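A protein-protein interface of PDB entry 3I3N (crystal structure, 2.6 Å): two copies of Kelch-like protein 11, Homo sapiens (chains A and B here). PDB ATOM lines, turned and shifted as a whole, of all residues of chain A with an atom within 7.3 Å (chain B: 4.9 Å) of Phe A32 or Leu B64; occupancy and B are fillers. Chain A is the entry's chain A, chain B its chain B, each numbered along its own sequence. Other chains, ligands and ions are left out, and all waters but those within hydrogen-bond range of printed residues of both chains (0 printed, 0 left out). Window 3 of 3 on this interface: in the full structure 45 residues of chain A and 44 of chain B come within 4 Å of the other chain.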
ATOM      1  N   GLN A  26     -17.252 -13.892  34.620  1.00  0.00           N
ATOM      2  CA  GLN A  26     -17.116 -13.975  33.172  1.00  0.00           C
ATOM      3  C   GLN A  26     -17.837 -12.831  32.503  1.00  0.00           C
ATOM      4  O   GLN A  26     -17.316 -12.209  31.578  1.00  0.00           O
ATOM      5  CB  GLN A  26     -17.697 -15.281  32.659  1.00  0.00           C
ATOM      6  CG  GLN A  26     -16.898 -16.505  33.025  1.00  0.00           C
ATOM      7  CD  GLN A  26     -17.634 -17.783  32.689  1.00  0.00           C
ATOM      8  OE1 GLN A  26     -18.625 -17.773  31.939  1.00  0.00           O
ATOM      9  NE2 GLN A  26     -17.156 -18.896  33.241  1.00  0.00           N
ATOM     10  N   ARG A  27     -19.054 -12.564  32.964  1.00  0.00           N
ATOM     11  CA  ARG A  27     -19.853 -11.501  32.394  1.00  0.00           C
ATOM     12  C   ARG A  27     -19.039 -10.227  32.375  1.00  0.00           C
ATOM     13  O   ARG A  27     -18.928  -9.557  31.348  1.00  0.00           O
ATOM     14  CB  ARG A  27     -21.116 -11.278  33.226  1.00  0.00           C
ATOM     15  CG  ARG A  27     -22.003 -10.193  32.685  1.00  0.00           C
ATOM     16  CD  ARG A  27     -23.252 -10.059  33.515  1.00  0.00           C
ATOM     17  NE  ARG A  27     -22.951  -9.593  34.864  1.00  0.00           N
ATOM     18  CZ  ARG A  27     -22.645  -8.332  35.170  1.00  0.00           C
ATOM     19  NH1 ARG A  27     -22.598  -7.392  34.230  1.00  0.00           N
ATOM     20  NH2 ARG A  27     -22.395  -8.006  36.427  1.00  0.00           N
ATOM     21  N   GLN A  29     -15.953  -9.746  32.328  1.00  0.00           N
ATOM     22  CA  GLN A  29     -14.802  -9.734  31.431  1.00  0.00           C
ATOM     23  C   GLN A  29     -15.237  -9.925  29.979  1.00  0.00           C
ATOM     24  O   GLN A  29     -14.405  -9.937  29.073  1.00  0.00           O
ATOM     25  CB  GLN A  29     -13.821 -10.830  31.831  1.00  0.00           C
ATOM     26  CG  GLN A  29     -13.429 -10.748  33.294  1.00  0.00           C
ATOM     27  CD  GLN A  29     -12.571 -11.918  33.742  1.00  0.00           C
ATOM     28  OE1 GLN A  29     -11.483 -12.146  33.201  1.00  0.00           O
ATOM     29  NE2 GLN A  29     -13.052 -12.668  34.740  1.00  0.00           N
ATOM     30  N   GLY A  30     -16.541 -10.049  29.756  1.00  0.00           N
ATOM     31  CA  GLY A  30     -17.040 -10.257  28.407  1.00  0.00           C
ATOM     32  C   GLY A  30     -16.720 -11.660  27.894  1.00  0.00           C
ATOM     33  O   GLY A  30     -16.721 -11.904  26.684  1.00  0.00           O
ATOM     34  N   LEU A  31     -16.441 -12.581  28.818  1.00  0.00           N
ATOM     35  CA  LEU A  31     -16.108 -13.962  28.478  1.00  0.00           C
ATOM     36  C   LEU A  31     -17.326 -14.861  28.232  1.00  0.00           C
ATOM     37  O   LEU A  31     -18.224 -14.981  29.080  1.00  0.00           O
ATOM     38  CB  LEU A  31     -15.250 -14.578  29.582  1.00  0.00           C
ATOM     39  CG  LEU A  31     -13.869 -13.971  29.855  1.00  0.00           C
ATOM     40  CD1 LEU A  31     -13.179 -14.799  30.924  1.00  0.00           C
ATOM     41  CD2 LEU A  31     -13.018 -13.942  28.587  1.00  0.00           C
ATOM     42  N   PHE A  32     -17.332 -15.496  27.065  1.00  0.00           N
ATOM     43  CA  PHE A  32     -18.402 -16.396  26.660  1.00  0.00           C
ATOM     44  C   PHE A  32     -19.741 -15.713  26.512  1.00  0.00           C
ATOM     45  O   PHE A  32     -20.750 -16.402  26.385  1.00  0.00           O
ATOM     46  CB  PHE A  32     -18.566 -17.535  27.667  1.00  0.00           C
ATOM     47  CG  PHE A  32     -17.337 -18.383  27.836  1.00  0.00           C
ATOM     48  CD1 PHE A  32     -16.889 -19.197  26.806  1.00  0.00           C
ATOM     49  CD2 PHE A  32     -16.624 -18.366  29.031  1.00  0.00           C
ATOM     50  CE1 PHE A  32     -15.747 -19.986  26.968  1.00  0.00           C
ATOM     51  CE2 PHE A  32     -15.480 -19.154  29.201  1.00  0.00           C
ATOM     52  CZ  PHE A  32     -15.041 -19.966  28.167  1.00  0.00           C
ATOM     53  N   CYS A  33     -19.780 -14.381  26.541  1.00  0.00           N
ATOM     54  CA  CYS A  33     -21.065 -13.693  26.416  1.00  0.00           C
ATOM     55  C   CYS A  33     -21.614 -13.889  25.017  1.00  0.00           C
ATOM     56  O   CYS A  33     -20.856 -13.988  24.053  1.00  0.00           O
ATOM     57  CB  CYS A  33     -20.918 -12.214  26.754  1.00  0.00           C
ATOM     58  SG  CYS A  33     -20.556 -11.971  28.502  1.00  0.00           S
ATOM     59  N   ASP A  34     -22.932 -13.947  24.905  1.00  0.00           N
ATOM     60  CA  ASP A  34     -23.549 -14.207  23.620  1.00  0.00           C
ATOM     61  C   ASP A  34     -24.747 -13.320  23.337  1.00  0.00           C
ATOM     62  O   ASP A  34     -25.569 -13.608  22.464  1.00  0.00           O
ATOM     63  CB  ASP A  34     -23.949 -15.693  23.558  1.00  0.00           C
ATOM     64  CG  ASP A  34     -25.002 -16.077  24.610  1.00  0.00           C
ATOM     65  OD1 ASP A  34     -25.190 -15.341  25.614  1.00  0.00           O
ATOM     66  OD2 ASP A  34     -25.639 -17.140  24.430  1.00  0.00           O
ATOM     67  N   ILE A  35     -24.863 -12.243  24.091  1.00  0.00           N
ATOM     68  CA  ILE A  35     -25.947 -11.320  23.868  1.00  0.00           C
ATOM     69  C   ILE A  35     -25.516  -9.973  24.416  1.00  0.00           C
ATOM     70  O   ILE A  35     -24.555  -9.877  25.193  1.00  0.00           O
ATOM     71  CB  ILE A  35     -27.260 -11.797  24.527  1.00  0.00           C
ATOM     72  CG1 ILE A  35     -28.430 -10.979  23.978  1.00  0.00           C
ATOM     73  CG2 ILE A  35     -27.172 -11.678  26.029  1.00  0.00           C
ATOM     74  CD1 ILE A  35     -29.793 -11.350  24.557  1.00  0.00           C
ATOM     75  N   ARG A  48     -22.902  -6.652  28.097  1.00  0.00           N
ATOM     76  CA  ARG A  48     -22.744  -8.031  27.650  1.00  0.00           C
ATOM     77  C   ARG A  48     -23.250  -8.984  28.729  1.00  0.00           C
ATOM     78  O   ARG A  48     -23.187  -8.672  29.920  1.00  0.00           O
ATOM     79  CB  ARG A  48     -21.279  -8.320  27.312  1.00  0.00           C
ATOM     80  CG  ARG A  48     -20.777  -7.498  26.114  1.00  0.00           C
ATOM     81  CD  ARG A  48     -19.457  -8.001  25.517  1.00  0.00           C
ATOM     82  NE  ARG A  48     -19.536  -9.325  24.875  1.00  0.00           N
ATOM     83  CZ  ARG A  48     -20.483  -9.711  24.014  1.00  0.00           C
ATOM     84  NH1 ARG A  48     -21.473  -8.889  23.675  1.00  0.00           N
ATOM     85  NH2 ARG A  48     -20.420 -10.914  23.455  1.00  0.00           N
ATOM     86  N   ALA A  49     -23.776 -10.132  28.298  1.00  0.00           N
ATOM     87  CA  ALA A  49     -24.324 -11.128  29.204  1.00  0.00           C
ATOM     88  C   ALA A  49     -24.571 -12.470  28.485  1.00  0.00           C
ATOM     89  O   ALA A  49     -24.517 -12.549  27.260  1.00  0.00           O
ATOM     90  CB  ALA A  49     -25.621 -10.610  29.776  1.00  0.00           C
ATOM     91  N   HIS A  50     -24.855 -13.513  29.260  1.00  0.00           N
ATOM     92  CA  HIS A  50     -25.130 -14.833  28.707  1.00  0.00           C
ATOM     93  C   HIS A  50     -26.623 -15.077  28.653  1.00  0.00           C
ATOM     94  O   HIS A  50     -27.318 -14.863  29.651  1.00  0.00           O
ATOM     95  CB  HIS A  50     -24.504 -15.933  29.566  1.00  0.00           C
ATOM     96  CG  HIS A  50     -23.071 -15.695  29.906  1.00  0.00           C
ATOM     97  ND1 HIS A  50     -22.680 -14.904  30.966  1.00  0.00           N
ATOM     98  CD2 HIS A  50     -21.934 -16.137  29.324  1.00  0.00           C
ATOM     99  CE1 HIS A  50     -21.361 -14.874  31.024  1.00  0.00           C
ATOM    100  NE2 HIS A  50     -20.884 -15.614  30.039  1.00  0.00           N
ATOM    101  N   ARG A  51     -27.105 -15.545  27.500  1.00  0.00           N
ATOM    102  CA  ARG A  51     -28.532 -15.839  27.314  1.00  0.00           C
ATOM    103  C   ARG A  51     -29.036 -16.904  28.271  1.00  0.00           C
ATOM    104  O   ARG A  51     -30.169 -16.843  28.758  1.00  0.00           O
ATOM    105  CB  ARG A  51     -28.804 -16.321  25.888  1.00  0.00           C
ATOM    106  CG  ARG A  51     -28.581 -15.281  24.803  1.00  0.00           C
ATOM    107  CD  ARG A  51     -28.185 -15.964  23.486  1.00  0.00           C
ATOM    108  NE  ARG A  51     -29.301 -16.575  22.764  1.00  0.00           N
ATOM    109  CZ  ARG A  51     -29.192 -17.646  21.971  1.00  0.00           C
ATOM    110  NH1 ARG A  51     -28.015 -18.252  21.803  1.00  0.00           N
ATOM    111  NH2 ARG A  51     -30.254 -18.087  21.303  1.00  0.00           N
ATOM    112  N   ILE B  35     -22.200 -25.489  22.404  1.00  0.00           N
ATOM    113  CA  ILE B  35     -21.101 -26.416  22.328  1.00  0.00           C
ATOM    114  C   ILE B  35     -21.704 -27.790  22.414  1.00  0.00           C
ATOM    115  O   ILE B  35     -22.663 -28.009  23.161  1.00  0.00           O
ATOM    116  CB  ILE B  35     -20.078 -26.162  23.451  1.00  0.00           C
ATOM    117  CG1 ILE B  35     -18.952 -27.179  23.341  1.00  0.00           C
ATOM    118  CG2 ILE B  35     -20.762 -26.206  24.819  1.00  0.00           C
ATOM    119  CD1 ILE B  35     -17.748 -26.850  24.210  1.00  0.00           C
ATOM    120  N   ARG B  51     -21.163 -23.222  27.168  1.00  0.00           N
ATOM    121  CA  ARG B  51     -19.748 -22.940  27.443  1.00  0.00           C
ATOM    122  C   ARG B  51     -19.546 -22.229  28.770  1.00  0.00           C
ATOM    123  O   ARG B  51     -18.643 -22.566  29.533  1.00  0.00           O
ATOM    124  CB  ARG B  51     -19.142 -22.051  26.365  1.00  0.00           C
ATOM    125  CG  ARG B  51     -19.090 -22.648  24.998  1.00  0.00           C
ATOM    126  CD  ARG B  51     -18.611 -21.621  23.997  1.00  0.00           C
ATOM    127  NE  ARG B  51     -18.636 -22.172  22.645  1.00  0.00           N
ATOM    128  CZ  ARG B  51     -17.580 -22.687  22.019  1.00  0.00           C
ATOM    129  NH1 ARG B  51     -16.393 -22.710  22.619  1.00  0.00           N
ATOM    130  NH2 ARG B  51     -17.718 -23.213  20.806  1.00  0.00           N
ATOM    131  N   SER B  52     -20.372 -21.229  29.031  1.00  0.00           N
ATOM    132  CA  SER B  52     -20.261 -20.472  30.261  1.00  0.00           C
ATOM    133  C   SER B  52     -20.301 -21.372  31.472  1.00  0.00           C
ATOM    134  O   SER B  52     -19.563 -21.152  32.423  1.00  0.00           O
ATOM    135  CB  SER B  52     -21.387 -19.442  30.346  1.00  0.00           C
ATOM    136  OG  SER B  52     -21.717 -19.192  31.692  1.00  0.00           O
ATOM    137  N   ALA B  55     -17.010 -23.887  31.479  1.00  0.00           N
ATOM    138  CA  ALA B  55     -15.816 -23.158  31.938  1.00  0.00           C
ATOM    139  C   ALA B  55     -15.897 -22.781  33.420  1.00  0.00           C
ATOM    140  O   ALA B  55     -14.885 -22.748  34.107  1.00  0.00           O
ATOM    141  CB  ALA B  55     -15.605 -21.909  31.095  1.00  0.00           C
ATOM    142  N   PHE B  61     -12.073 -26.457  30.612  1.00  0.00           N
ATOM    143  CA  PHE B  61     -12.738 -25.873  29.453  1.00  0.00           C
ATOM    144  C   PHE B  61     -12.425 -24.405  29.171  1.00  0.00           C
ATOM    145  O   PHE B  61     -12.780 -23.892  28.117  1.00  0.00           O
ATOM    146  CB  PHE B  61     -14.248 -26.060  29.579  1.00  0.00           C
ATOM    147  CG  PHE B  61     -14.696 -27.467  29.343  1.00  0.00           C
ATOM    148  CD1 PHE B  61     -14.512 -28.069  28.100  1.00  0.00           C
ATOM    149  CD2 PHE B  61     -15.306 -28.196  30.352  1.00  0.00           C
ATOM    150  CE1 PHE B  61     -14.928 -29.377  27.874  1.00  0.00           C
ATOM    151  CE2 PHE B  61     -15.722 -29.509  30.126  1.00  0.00           C
ATOM    152  CZ  PHE B  61     -15.535 -30.093  28.890  1.00  0.00           C
ATOM    153  N   THR B  62     -11.775 -23.721  30.099  1.00  0.00           N
ATOM    154  CA  THR B  62     -11.425 -22.329  29.856  1.00  0.00           C
ATOM    155  C   THR B  62     -10.589 -22.230  28.571  1.00  0.00           C
ATOM    156  O   THR B  62     -10.816 -21.351  27.744  1.00  0.00           O
ATOM    157  CB  THR B  62     -10.627 -21.727  31.041  1.00  0.00           C
ATOM    158  OG1 THR B  62     -11.457 -21.695  32.211  1.00  0.00           O
ATOM    159  CG2 THR B  62     -10.169 -20.308  30.712  1.00  0.00           C
ATOM    160  N   PRO B  63      -9.620 -23.152  28.383  1.00  0.00           N
ATOM    161  CA  PRO B  63      -8.741 -23.187  27.207  1.00  0.00           C
ATOM    162  C   PRO B  63      -9.444 -23.359  25.868  1.00  0.00           C
ATOM    163  O   PRO B  63      -8.788 -23.549  24.844  1.00  0.00           O
ATOM    164  CB  PRO B  63      -7.820 -24.367  27.499  1.00  0.00           C
ATOM    165  CG  PRO B  63      -7.735 -24.358  28.984  1.00  0.00           C
ATOM    166  CD  PRO B  63      -9.179 -24.159  29.364  1.00  0.00           C
ATOM    167  N   LEU B  64     -10.773 -23.308  25.868  1.00  0.00           N
ATOM    168  CA  LEU B  64     -11.503 -23.460  24.618  1.00  0.00           C
ATOM    169  C   LEU B  64     -11.897 -22.105  24.050  1.00  0.00           C
ATOM    170  O   LEU B  64     -12.604 -22.027  23.041  1.00  0.00           O
ATOM    171  CB  LEU B  64     -12.750 -24.342  24.797  1.00  0.00           C
ATOM    172  CG  LEU B  64     -14.000 -23.913  25.565  1.00  0.00           C
ATOM    173  CD1 LEU B  64     -14.602 -22.668  24.955  1.00  0.00           C
ATOM    174  CD2 LEU B  64     -15.010 -25.048  25.527  1.00  0.00           C
ATOM    175  N   LEU B  65     -11.462 -21.037  24.719  1.00  0.00           N
ATOM    176  CA  LEU B  65     -11.738 -19.680  24.256  1.00  0.00           C
ATOM    177  C   LEU B  65     -10.760 -19.433  23.122  1.00  0.00           C
ATOM    178  O   LEU B  65     -11.149 -19.185  21.977  1.00  0.00           O
ATOM    179  CB  LEU B  65     -11.478 -18.654  25.363  1.00  0.00           C
ATOM    180  CG  LEU B  65     -12.597 -18.341  26.360  1.00  0.00           C
ATOM    181  CD1 LEU B  65     -12.015 -17.593  27.544  1.00  0.00           C
ATOM    182  CD2 LEU B  65     -13.694 -17.524  25.683  1.00  0.00           C
ATOM    183  N   SER B  66      -9.481 -19.521  23.465  1.00  0.00           N
ATOM    184  CA  SER B  66      -8.393 -19.323  22.520  1.00  0.00           C
ATOM    185  C   SER B  66      -8.612 -20.098  21.220  1.00  0.00           C
ATOM    186  O   SER B  66      -8.178 -19.665  20.152  1.00  0.00           O
ATOM    187  CB  SER B  66      -7.082 -19.758  23.167  1.00  0.00           C
ATOM    188  OG  SER B  66      -6.956 -19.176  24.453  1.00  0.00           O
ATOM    189  N   GLY B  67      -9.288 -21.240  21.320  1.00  0.00           N
ATOM    190  CA  GLY B  67      -9.550 -22.057  20.150  1.00  0.00           C
ATOM    191  C   GLY B  67      -8.683 -23.298  20.164  1.00  0.00           C
ATOM    192  O   GLY B  67      -8.261 -23.783  19.117  1.00  0.00           O
ATOM    193  N   GLN B  68      -8.419 -23.814  21.361  1.00  0.00           N
ATOM    194  CA  GLN B  68      -7.588 -25.001  21.508  1.00  0.00           C
ATOM    195  C   GLN B  68      -8.343 -26.299  21.282  1.00  0.00           C
ATOM    196  O   GLN B  68      -7.797 -27.380  21.495  1.00  0.00           O
ATOM    197  CB  GLN B  68      -6.933 -25.028  22.886  1.00  0.00           C
ATOM    198  CG  GLN B  68      -5.872 -23.960  23.076  1.00  0.00           C
ATOM    199  CD  GLN B  68      -4.991 -24.227  24.283  1.00  0.00           C
ATOM    200  OE1 GLN B  68      -4.095 -23.440  24.595  1.00  0.00           O
ATOM    201  NE2 GLN B  68      -5.239 -25.345  24.970  1.00  0.00           N
ATOM    202  N   PHE B  69      -9.597 -26.196  20.857  1.00  0.00           N
ATOM    203  CA  PHE B  69     -10.399 -27.386  20.589  1.00  0.00           C
ATOM    204  C   PHE B  69     -10.778 -27.429  19.105  1.00  0.00           C
ATOM    205  O   PHE B  69     -10.936 -26.386  18.464  1.00  0.00           O
ATOM    206  CB  PHE B  69     -11.664 -27.397  21.463  1.00  0.00           C
ATOM    207  CG  PHE B  69     -11.400 -27.649  22.938  1.00  0.00           C
ATOM    208  CD1 PHE B  69     -10.734 -26.706  23.719  1.00  0.00           C
ATOM    209  CD2 PHE B  69     -11.835 -28.827  23.544  1.00  0.00           C
ATOM    210  CE1 PHE B  69     -10.508 -26.932  25.084  1.00  0.00           C
ATOM    211  CE2 PHE B  69     -11.616 -29.064  24.900  1.00  0.00           C
ATOM    212  CZ  PHE B  69     -10.951 -28.113  25.673  1.00  0.00           C
ATOM    213  N   GLU B  71     -13.160 -27.315  16.917  1.00  0.00           N
ATOM    214  CA  GLU B  71     -14.565 -26.963  16.797  1.00  0.00           C
ATOM    215  C   GLU B  71     -15.056 -26.736  15.390  1.00  0.00           C
ATOM    216  O   GLU B  71     -14.443 -25.959  14.623  1.00  0.00           O
ATOM    217  CB  GLU B  71     -14.869 -25.708  17.600  1.00  0.00           C
ATOM    218  CG  GLU B  71     -14.371 -25.704  19.038  1.00  0.00           C
ATOM    219  CD  GLU B  71     -14.348 -24.320  19.666  1.00  0.00           C
ATOM    220  OE1 GLU B  71     -15.382 -23.623  19.603  1.00  0.00           O
ATOM    221  OE2 GLU B  71     -13.296 -23.936  20.228  1.00  0.00           O
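Phe A32 touches just these residues of chain B: Arg B51, Ala B55, Leu B64 and Leu B65.
Printed residues of chain A within 4 Å of Leu B64: Phe A32.
Printed residues of chain A within 4 Å of Ala B55: Phe A32 (3.3 Å).
Of the printed residues of chain A, Arg B51 touches Phe A32 (3.7 Å).
Of the printed residues of chain B, Gln A26 touches Ser B52 (3.4 Å).
Printed residues of chain B within 4 Å of Leu A31: Leu B65 (3.9 Å).
Of the printed residues of chain A, Leu B65 touches Leu A31 (3.9 Å) and Phe A32 (3.4 Å).
Phe B61 touches none of the printed residues of chain A.
The nearest residue of chain B that does not touch Phe A32 is Ser B52 (4.3 Å).
The nearest printed residue of chain A that does not touch Leu B64 is Leu A31 (8.9 Å).
The nearest printed residue of chain B that does not touch His A50 is Arg B51 (6.6 Å).
Among the printed residues, pairs that only touch across the chains: Phe A32 with Ala B55 (3.3 Å), Phe A32 with Leu B65 (3.4 Å), His A50 with Ser B52 (3.5 Å), Phe A32 with Leu B64 (3.5 Å), Phe A32 with Arg B51 (3.7 Å) and Leu A31 with Leu B65 (3.9 Å).
NE2 of Gln A26 is in hydrogen-bond range of O of Ser B52.
O of Gln A26 sits at hydrogen-bond distance from N of Leu A31.
NE2 of His A50 is in hydrogen-bond range of O of Leu A31 (2.9 Å).
The side-chain carboxylate (OE1) of Glu B71 lies within salt-bridge range of the guanidinium group (NH2) of Arg B51, at 2.7 Å.
Of the 13 printed residues of chain A, 4 touch a printed residue of chain B.
Hydrophobic or aromatic side chains of chain A that line the printed part of chain B: Leu A31, Phe A32 and His A50.
Along chain A the printed residues that touch a printed residue of chain B span positions 26 to 50.
Of the 14 printed residues of chain B, 5 touch a printed residue of chain A.
Hydrophobic or aromatic side chains of chain B that line the printed part of chain A: Ala B55, Leu B64 and Leu B65.
Among the printed residues, 7 pairs touch across the chains.
Among the printed residues, no Asp or Glu carboxylate lies within 4 Å of a Lys or Arg side-chain nitrogen of the other chain.
2 positions are printed for both chains.
Of the 7 pairs that touch across the chains among the printed residues, none has its exchanged pair printed and touching as well.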
